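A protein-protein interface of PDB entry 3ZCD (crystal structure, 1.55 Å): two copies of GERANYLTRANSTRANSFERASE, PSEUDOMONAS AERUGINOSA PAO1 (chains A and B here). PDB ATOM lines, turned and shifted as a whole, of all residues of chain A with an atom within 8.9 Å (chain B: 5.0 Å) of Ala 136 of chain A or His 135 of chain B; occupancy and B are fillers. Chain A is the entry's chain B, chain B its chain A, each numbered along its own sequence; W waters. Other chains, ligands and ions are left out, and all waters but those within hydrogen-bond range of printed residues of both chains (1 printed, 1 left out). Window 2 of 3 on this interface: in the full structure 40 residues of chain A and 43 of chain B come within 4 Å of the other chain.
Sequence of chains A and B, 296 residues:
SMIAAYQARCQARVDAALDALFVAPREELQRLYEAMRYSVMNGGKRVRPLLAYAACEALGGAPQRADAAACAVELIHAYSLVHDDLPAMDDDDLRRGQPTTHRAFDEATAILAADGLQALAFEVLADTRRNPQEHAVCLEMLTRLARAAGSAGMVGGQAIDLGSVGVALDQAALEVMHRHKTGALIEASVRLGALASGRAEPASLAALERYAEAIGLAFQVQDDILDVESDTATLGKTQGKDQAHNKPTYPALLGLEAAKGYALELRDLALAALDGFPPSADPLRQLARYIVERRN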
ATOM      1  N   ALA A 126      27.430  25.887  -0.247  1.00  0.00           N
ATOM      2  CA  ALA A 126      26.928  24.778  -1.032  1.00  0.00           C
ATOM      3  C   ALA A 126      26.684  23.520  -0.201  1.00  0.00           C
ATOM      4  O   ALA A 126      26.039  22.591  -0.677  1.00  0.00           O
ATOM      5  CB  ALA A 126      27.930  24.477  -2.162  1.00  0.00           C
ATOM      6  N   THR A 128      24.880  21.534   2.274  1.00  0.00           N
ATOM      7  CA  THR A 128      23.493  21.633   2.782  1.00  0.00           C
ATOM      8  C   THR A 128      23.356  21.137   4.242  1.00  0.00           C
ATOM      9  O   THR A 128      22.309  21.295   4.822  1.00  0.00           O
ATOM     10  CB  THR A 128      22.513  20.901   1.843  1.00  0.00           C
ATOM     11  OG1 THR A 128      22.870  19.529   1.761  1.00  0.00           O
ATOM     12  CG2 THR A 128      22.530  21.518   0.459  1.00  0.00           C
ATOM     13  N   ASN A 131      24.664  24.708   5.659  1.00  0.00           N
ATOM     14  CA  ASN A 131      23.755  25.739   5.131  1.00  0.00           C
ATOM     15  C   ASN A 131      22.450  25.100   4.713  1.00  0.00           C
ATOM     16  O   ASN A 131      22.130  25.012   3.527  1.00  0.00           O
ATOM     17  CB  ASN A 131      24.399  26.476   3.918  1.00  0.00           C
ATOM     18  CG  ASN A 131      23.597  27.711   3.476  1.00  0.00           C
ATOM     19  OD1 ASN A 131      22.958  28.375   4.301  1.00  0.00           O
ATOM     20  ND2 ASN A 131      23.617  28.040   2.187  1.00  0.00           N
ATOM     21  N   GLN A 133      19.360  25.437   3.946  1.00  0.00           N
ATOM     22  CA  GLN A 133      18.284  26.157   3.262  1.00  0.00           C
ATOM     23  C   GLN A 133      17.710  25.279   2.160  1.00  0.00           C
ATOM     24  O   GLN A 133      18.316  24.264   1.796  1.00  0.00           O
ATOM     25  CB  GLN A 133      18.750  27.485   2.652  1.00  0.00           C
ATOM     26  CG  GLN A 133      19.779  28.264   3.447  1.00  0.00           C
ATOM     27  CD  GLN A 133      19.466  28.474   4.926  1.00  0.00           C
ATOM     28  OE1 GLN A 133      18.312  28.627   5.291  1.00  0.00           O
ATOM     29  NE2 GLN A 133      20.486  28.437   5.779  1.00  0.00           N
ATOM     30  N   GLU A 134      16.547  25.659   1.619  1.00  0.00           N
ATOM     31  CA  GLU A 134      16.045  25.049   0.386  1.00  0.00           C
ATOM     32  C   GLU A 134      17.153  25.207  -0.718  1.00  0.00           C
ATOM     33  O   GLU A 134      17.794  26.232  -0.809  1.00  0.00           O
ATOM     34  CB  GLU A 134      14.770  25.718  -0.071  1.00  0.00           C
ATOM     35  CG  GLU A 134      13.599  25.526   0.919  1.00  0.00           C
ATOM     36  CD  GLU A 134      12.793  24.244   0.733  1.00  0.00           C
ATOM     37  OE1 GLU A 134      13.319  23.129   1.007  1.00  0.00           O
ATOM     38  OE2 GLU A 134      11.596  24.355   0.356  1.00  0.00           O
ATOM     39  N   HIS A 135      17.268  24.209  -1.569  1.00  0.00           N
ATOM     40  CA  HIS A 135      18.357  24.186  -2.569  1.00  0.00           C
ATOM     41  C   HIS A 135      18.320  25.408  -3.468  1.00  0.00           C
ATOM     42  O   HIS A 135      19.368  25.995  -3.733  1.00  0.00           O
ATOM     43  CB  HIS A 135      18.247  22.907  -3.380  1.00  0.00           C
ATOM     44  CG  HIS A 135      18.580  21.676  -2.592  1.00  0.00           C
ATOM     45  ND1 HIS A 135      18.490  20.409  -3.111  1.00  0.00           N
ATOM     46  CD2 HIS A 135      18.996  21.525  -1.308  1.00  0.00           C
ATOM     47  CE1 HIS A 135      18.850  19.531  -2.194  1.00  0.00           C
ATOM     48  NE2 HIS A 135      19.181  20.184  -1.099  1.00  0.00           N
ATOM     49  N   ALA A 136      17.138  25.866  -3.905  1.00  0.00           N
ATOM     50  CA  ALA A 136      17.086  27.087  -4.731  1.00  0.00           C
ATOM     51  C   ALA A 136      17.638  28.323  -4.007  1.00  0.00           C
ATOM     52  O   ALA A 136      18.276  29.193  -4.629  1.00  0.00           O
ATOM     53  CB  ALA A 136      15.698  27.359  -5.203  1.00  0.00           C
ATOM     54  N   VAL A 137      17.381  28.386  -2.697  1.00  0.00           N
ATOM     55  CA  VAL A 137      17.877  29.447  -1.860  1.00  0.00           C
ATOM     56  C   VAL A 137      19.410  29.329  -1.728  1.00  0.00           C
ATOM     57  O   VAL A 137      20.094  30.351  -1.771  1.00  0.00           O
ATOM     58  CB  VAL A 137      17.175  29.470  -0.497  1.00  0.00           C
ATOM     59  CG1 VAL A 137      17.837  30.447   0.450  1.00  0.00           C
ATOM     60  CG2 VAL A 137      15.718  29.841  -0.714  1.00  0.00           C
ATOM     61  N   CYS A 138      19.924  28.119  -1.516  1.00  0.00           N
ATOM     62  CA  CYS A 138      21.401  27.934  -1.436  1.00  0.00           C
ATOM     63  C   CYS A 138      22.028  28.469  -2.686  1.00  0.00           C
ATOM     64  O   CYS A 138      23.044  29.157  -2.606  1.00  0.00           O
ATOM     65  CB  CYS A 138      21.844  26.479  -1.216  1.00  0.00           C
ATOM     66  SG  CYS A 138      21.240  25.742   0.340  1.00  0.00           S
ATOM     67  N   LEU A 139      21.448  28.146  -3.830  1.00  0.00           N
ATOM     68  CA  LEU A 139      22.067  28.599  -5.150  1.00  0.00           C
ATOM     69  C   LEU A 139      22.014  30.111  -5.280  1.00  0.00           C
ATOM     70  O   LEU A 139      22.904  30.738  -5.800  1.00  0.00           O
ATOM     71  CB  LEU A 139      21.379  27.960  -6.345  1.00  0.00           C
ATOM     72  CG  LEU A 139      21.671  26.471  -6.488  1.00  0.00           C
ATOM     73  CD1 LEU A 139      20.793  25.841  -7.550  1.00  0.00           C
ATOM     74  CD2 LEU A 139      23.154  26.195  -6.777  1.00  0.00           C
ATOM     75  N   GLU A 140      20.928  30.735  -4.839  1.00  0.00           N
ATOM     76  CA  GLU A 140      20.832  32.179  -4.883  1.00  0.00           C
ATOM     77  C   GLU A 140      21.869  32.832  -3.949  1.00  0.00           C
ATOM     78  O   GLU A 140      22.438  33.854  -4.295  1.00  0.00           O
ATOM     79  CB  GLU A 140      19.398  32.653  -4.513  1.00  0.00           C
ATOM     80  CG  GLU A 140      19.234  34.157  -4.708  1.00  0.00           C
ATOM     81  CD  GLU A 140      19.483  34.729  -6.128  1.00  0.00           C
ATOM     82  OE1 GLU A 140      19.607  34.018  -7.179  1.00  0.00           O
ATOM     83  OE2 GLU A 140      19.558  35.979  -6.194  1.00  0.00           O
ATOM     84  N   MET A 141      22.127  32.227  -2.793  1.00  0.00           N
ATOM     85  CA  MET A 141      23.074  32.744  -1.836  1.00  0.00           C
ATOM     86  C   MET A 141      24.480  32.674  -2.514  1.00  0.00           C
ATOM     87  O   MET A 141      25.251  33.606  -2.456  1.00  0.00           O
ATOM     88  CB  MET A 141      23.100  31.933  -0.536  1.00  0.00           C
ATOM     89  CG  MET A 141      21.796  32.155   0.287  1.00  0.00           C
ATOM     90  SD  MET A 141      21.707  31.027   1.683  1.00  0.00           S
ATOM     91  CE  MET A 141      22.728  31.888   2.861  1.00  0.00           C
ATOM     92  N   LEU A 142      24.710  31.542  -3.116  1.00  0.00           N
ATOM     93  CA  LEU A 142      26.021  31.326  -3.821  1.00  0.00           C
ATOM     94  C   LEU A 142      26.172  32.304  -4.937  1.00  0.00           C
ATOM     95  O   LEU A 142      27.300  32.861  -5.168  1.00  0.00           O
ATOM     96  CB  LEU A 142      26.055  29.926  -4.384  1.00  0.00           C
ATOM     97  CG  LEU A 142      26.397  28.917  -3.303  1.00  0.00           C
ATOM     98  CD1 LEU A 142      25.720  27.583  -3.551  1.00  0.00           C
ATOM     99  CD2 LEU A 142      27.901  28.711  -3.274  1.00  0.00           C
ATOM    100  N   THR A 143      25.125  32.471  -5.704  1.00  0.00           N
ATOM    101  CA  THR A 143      25.149  33.381  -6.856  1.00  0.00           C
ATOM    102  C   THR A 143      25.479  34.801  -6.404  1.00  0.00           C
ATOM    103  O   THR A 143      26.353  35.507  -6.971  1.00  0.00           O
ATOM    104  CB  THR A 143      23.808  33.341  -7.623  1.00  0.00           C
ATOM    105  OG1 THR A 143      23.692  32.127  -8.365  1.00  0.00           O
ATOM    106  CG2 THR A 143      23.666  34.524  -8.549  1.00  0.00           C
ATOM    107  N   LEU A 195      18.092  35.888   2.952  1.00  0.00           N
ATOM    108  CA  LEU A 195      17.768  34.641   2.329  1.00  0.00           C
ATOM    109  C   LEU A 195      17.726  33.453   3.315  1.00  0.00           C
ATOM    110  O   LEU A 195      16.911  32.533   3.142  1.00  0.00           O
ATOM    111  CB  LEU A 195      18.735  34.358   1.179  1.00  0.00           C
ATOM    112  CG  LEU A 195      18.517  35.200  -0.078  1.00  0.00           C
ATOM    113  CD1 LEU A 195      19.734  35.097  -1.017  1.00  0.00           C
ATOM    114  CD2 LEU A 195      17.229  34.833  -0.821  1.00  0.00           C
ATOM    115  N   THR B 128      21.899  29.009 -12.744  1.00  0.00           N
ATOM    116  CA  THR B 128      21.070  27.941 -13.287  1.00  0.00           C
ATOM    117  C   THR B 128      20.688  28.144 -14.746  1.00  0.00           C
ATOM    118  O   THR B 128      20.112  27.238 -15.366  1.00  0.00           O
ATOM    119  CB  THR B 128      19.821  27.719 -12.419  1.00  0.00           C
ATOM    120  OG1 THR B 128      19.082  28.940 -12.314  1.00  0.00           O
ATOM    121  CG2 THR B 128      20.235  27.278 -11.047  1.00  0.00           C
ATOM    122  N   GLN B 133      21.259  22.289 -14.558  1.00  0.00           N
ATOM    123  CA  GLN B 133      21.041  20.976 -13.979  1.00  0.00           C
ATOM    124  C   GLN B 133      19.913  21.111 -12.956  1.00  0.00           C
ATOM    125  O   GLN B 133      19.560  22.209 -12.567  1.00  0.00           O
ATOM    126  CB  GLN B 133      22.315  20.431 -13.291  1.00  0.00           C
ATOM    127  CG  GLN B 133      23.631  20.708 -14.004  1.00  0.00           C
ATOM    128  CD  GLN B 133      23.619  20.339 -15.483  1.00  0.00           C
ATOM    129  OE1 GLN B 133      23.038  19.341 -15.892  1.00  0.00           O
ATOM    130  NE2 GLN B 133      24.281  21.159 -16.297  1.00  0.00           N
ATOM    131  N   GLU B 134      19.468  19.971 -12.462  1.00  0.00           N
ATOM    132  CA  GLU B 134      18.638  20.002 -11.248  1.00  0.00           C
ATOM    133  C   GLU B 134      19.420  20.659 -10.118  1.00  0.00           C
ATOM    134  O   GLU B 134      20.638  20.494  -9.958  1.00  0.00           O
ATOM    135  CB  GLU B 134      18.282  18.581 -10.852  1.00  0.00           C
ATOM    136  CG  GLU B 134      17.334  17.927 -11.822  1.00  0.00           C
ATOM    137  CD  GLU B 134      15.886  18.148 -11.423  1.00  0.00           C
ATOM    138  OE1 GLU B 134      15.613  18.850 -10.427  1.00  0.00           O
ATOM    139  OE2 GLU B 134      15.024  17.614 -12.113  1.00  0.00           O
ATOM    140  N   HIS B 135      18.739  21.417  -9.295  1.00  0.00           N
ATOM    141  CA  HIS B 135      19.392  22.200  -8.251  1.00  0.00           C
ATOM    142  C   HIS B 135      20.283  21.392  -7.313  1.00  0.00           C
ATOM    143  O   HIS B 135      21.357  21.838  -6.963  1.00  0.00           O
ATOM    144  CB  HIS B 135      18.378  23.018  -7.433  1.00  0.00           C
ATOM    145  CG  HIS B 135      17.696  24.090  -8.221  1.00  0.00           C
ATOM    146  ND1 HIS B 135      16.606  24.789  -7.743  1.00  0.00           N
ATOM    147  CD2 HIS B 135      17.893  24.532  -9.488  1.00  0.00           C
ATOM    148  CE1 HIS B 135      16.202  25.649  -8.660  1.00  0.00           C
ATOM    149  NE2 HIS B 135      16.966  25.511  -9.730  1.00  0.00           N
ATOM    150  N   ALA B 136      19.847  20.205  -6.914  1.00  0.00           N
ATOM    151  CA  ALA B 136      20.663  19.365  -6.065  1.00  0.00           C
ATOM    152  C   ALA B 136      21.994  18.999  -6.760  1.00  0.00           C
ATOM    153  O   ALA B 136      23.004  18.841  -6.088  1.00  0.00           O
ATOM    154  CB  ALA B 136      19.921  18.124  -5.688  1.00  0.00           C
ATOM    155  N   VAL B 137      21.918  18.795  -8.069  1.00  0.00           N
ATOM    156  CA  VAL B 137      23.090  18.455  -8.870  1.00  0.00           C
ATOM    157  C   VAL B 137      23.989  19.673  -8.981  1.00  0.00           C
ATOM    158  O   VAL B 137      25.222  19.540  -8.775  1.00  0.00           O
ATOM    159  CB  VAL B 137      22.705  17.903 -10.237  1.00  0.00           C
ATOM    160  CG1 VAL B 137      23.945  17.796 -11.107  1.00  0.00           C
ATOM    161  CG2 VAL B 137      22.046  16.538 -10.114  1.00  0.00           C
ATOM    162  N   CYS B 138      23.419  20.841  -9.221  1.00  0.00           N
ATOM    163  CA  CYS B 138      24.241  22.076  -9.176  1.00  0.00           C
ATOM    164  C   CYS B 138      25.017  22.216  -7.873  1.00  0.00           C
ATOM    165  O   CYS B 138      26.218  22.523  -7.835  1.00  0.00           O
ATOM    166  CB  CYS B 138      23.459  23.359  -9.402  1.00  0.00           C
ATOM    167  SG  CYS B 138      22.516  23.469 -10.911  1.00  0.00           S
ATOM    168  N   LEU B 139      24.338  22.011  -6.749  1.00  0.00           N
ATOM    169  CA  LEU B 139      25.000  22.112  -5.453  1.00  0.00           C
ATOM    170  C   LEU B 139      26.103  21.077  -5.244  1.00  0.00           C
ATOM    171  O   LEU B 139      27.132  21.367  -4.611  1.00  0.00           O
ATOM    172  CB  LEU B 139      23.976  21.985  -4.301  1.00  0.00           C
ATOM    173  CG  LEU B 139      23.104  23.222  -4.175  1.00  0.00           C
ATOM    174  CD1 LEU B 139      21.937  22.960  -3.177  1.00  0.00           C
ATOM    175  CD2 LEU B 139      23.845  24.473  -3.729  1.00  0.00           C
HETATM  176  O   HOH W   1      21.376  30.930 -10.302  1.00  0.00           O
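The backbone carbonyl oxygen of Gln 133 of chain B lies within hydrogen-bond range of the side-chain sulfur of Cys 138 of chain B. The backbone carbonyl oxygen of Glu 134 of chain B lies within hydrogen-bond range of the side-chain sulfur of Cys 138 of chain B (3.6 Å). O of Asn 131 of chain A lies within hydrogen-bond range of SG of Cys 138 of chain A (3.4 Å). SG of Cys 138 of chain A sits at hydrogen-bond distance from O of Gln 133 of chain A (3.6 Å). O of Glu 134 of chain A is in hydrogen-bond range of SG of Cys 138 of chain A. The backbone carbonyl oxygen (O) of Leu 139 of chain A lies within hydrogen-bond range of the side-chain hydroxyl (OG1) of Thr 143 of chain A (3.0 Å).
Thr 128 of chain A touches Leu 139 of chain B (CG2 to CD1, 3.96 Å). His 135 of chain A touches Ala 136 of chain B. His 135 of chain A touches Leu 139 of chain B (CG to CD1, 3.6 Å). His 135 of chain B touches Ala 136 of chain A (ND1 to CB, 3.7 Å). Cys 138 of chain A touches Leu 139 of chain B (CB to CD2, 3.8 Å). Thr 128 of chain B touches Leu 139 of chain A. Leu 139 of chain A touches His 135 of chain B. CD2 of Leu 139 of chain A touches CB of Cys 138 of chain B, at 3.9 Å. Leu 139 of chain A touches Leu 139 of chain B (CD2 to CD2, 3.6 Å). Leu 139 of chain B touches Leu 142 of chain A (CD2 to CD1, 3.6 Å).
Ala 136 of chain A touches just one residue of chain B: His 135 (3.7 Å). Of the printed residues of chain B, Leu 142 of chain A touches Leu 139. Printed residues of chain A within 4 Å of Thr 128 of chain B: Leu 139 (3.8 Å). Gln 133 of chain B touches none of the printed residues of chain A. Of chain A, only Ala 136 (3.7 Å) and Leu 139 (3.6 Å) come within 4 Å of His 135 of chain B. Ala 136 of chain B touches just one residue of chain A: His 135 (3.7 Å). The nearest printed residue of chain B that does not touch Ala 136 of chain A is Leu 139 of chain B (5.7 Å).
Hydrophobic or aromatic side chains of chain A within 4 Å of the printed part of chain B: His 135, Ala 136, Leu 139 and Leu 142. Of the 8 printed residues of chain B, 5 touch a printed residue of chain A. Hydrophobic or aromatic side chains of chain B that line the printed part of chain A: His 135, Ala 136 and Leu 139. Among the printed residues, 10 pairs touch across the chains. Among the printed residues, no Asp or Glu carboxylate lies within 4 Å of a Lys or Arg side-chain nitrogen of the other chain.
His 135 of chain A touches Ala 136 of chain B, and with the chains exchanged Ala 136 of chain A touches His 135 of chain B. His 135 of chain A touches Leu 139 of chain B, and with the chains exchanged Leu 139 of chain A touches His 135 of chain B. Cys 138 of chain A touches Leu 139 of chain B, and with the chains exchanged Leu 139 of chain A touches Cys 138 of chain B. Leu 139 of chain A touches its own counterpart, Leu 139 of chain B. 8 positions are printed for both chains.
Water W1 lies within hydrogen-bond range of N of Thr 128 of chain B and OG1 of Thr 143 of chain A.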
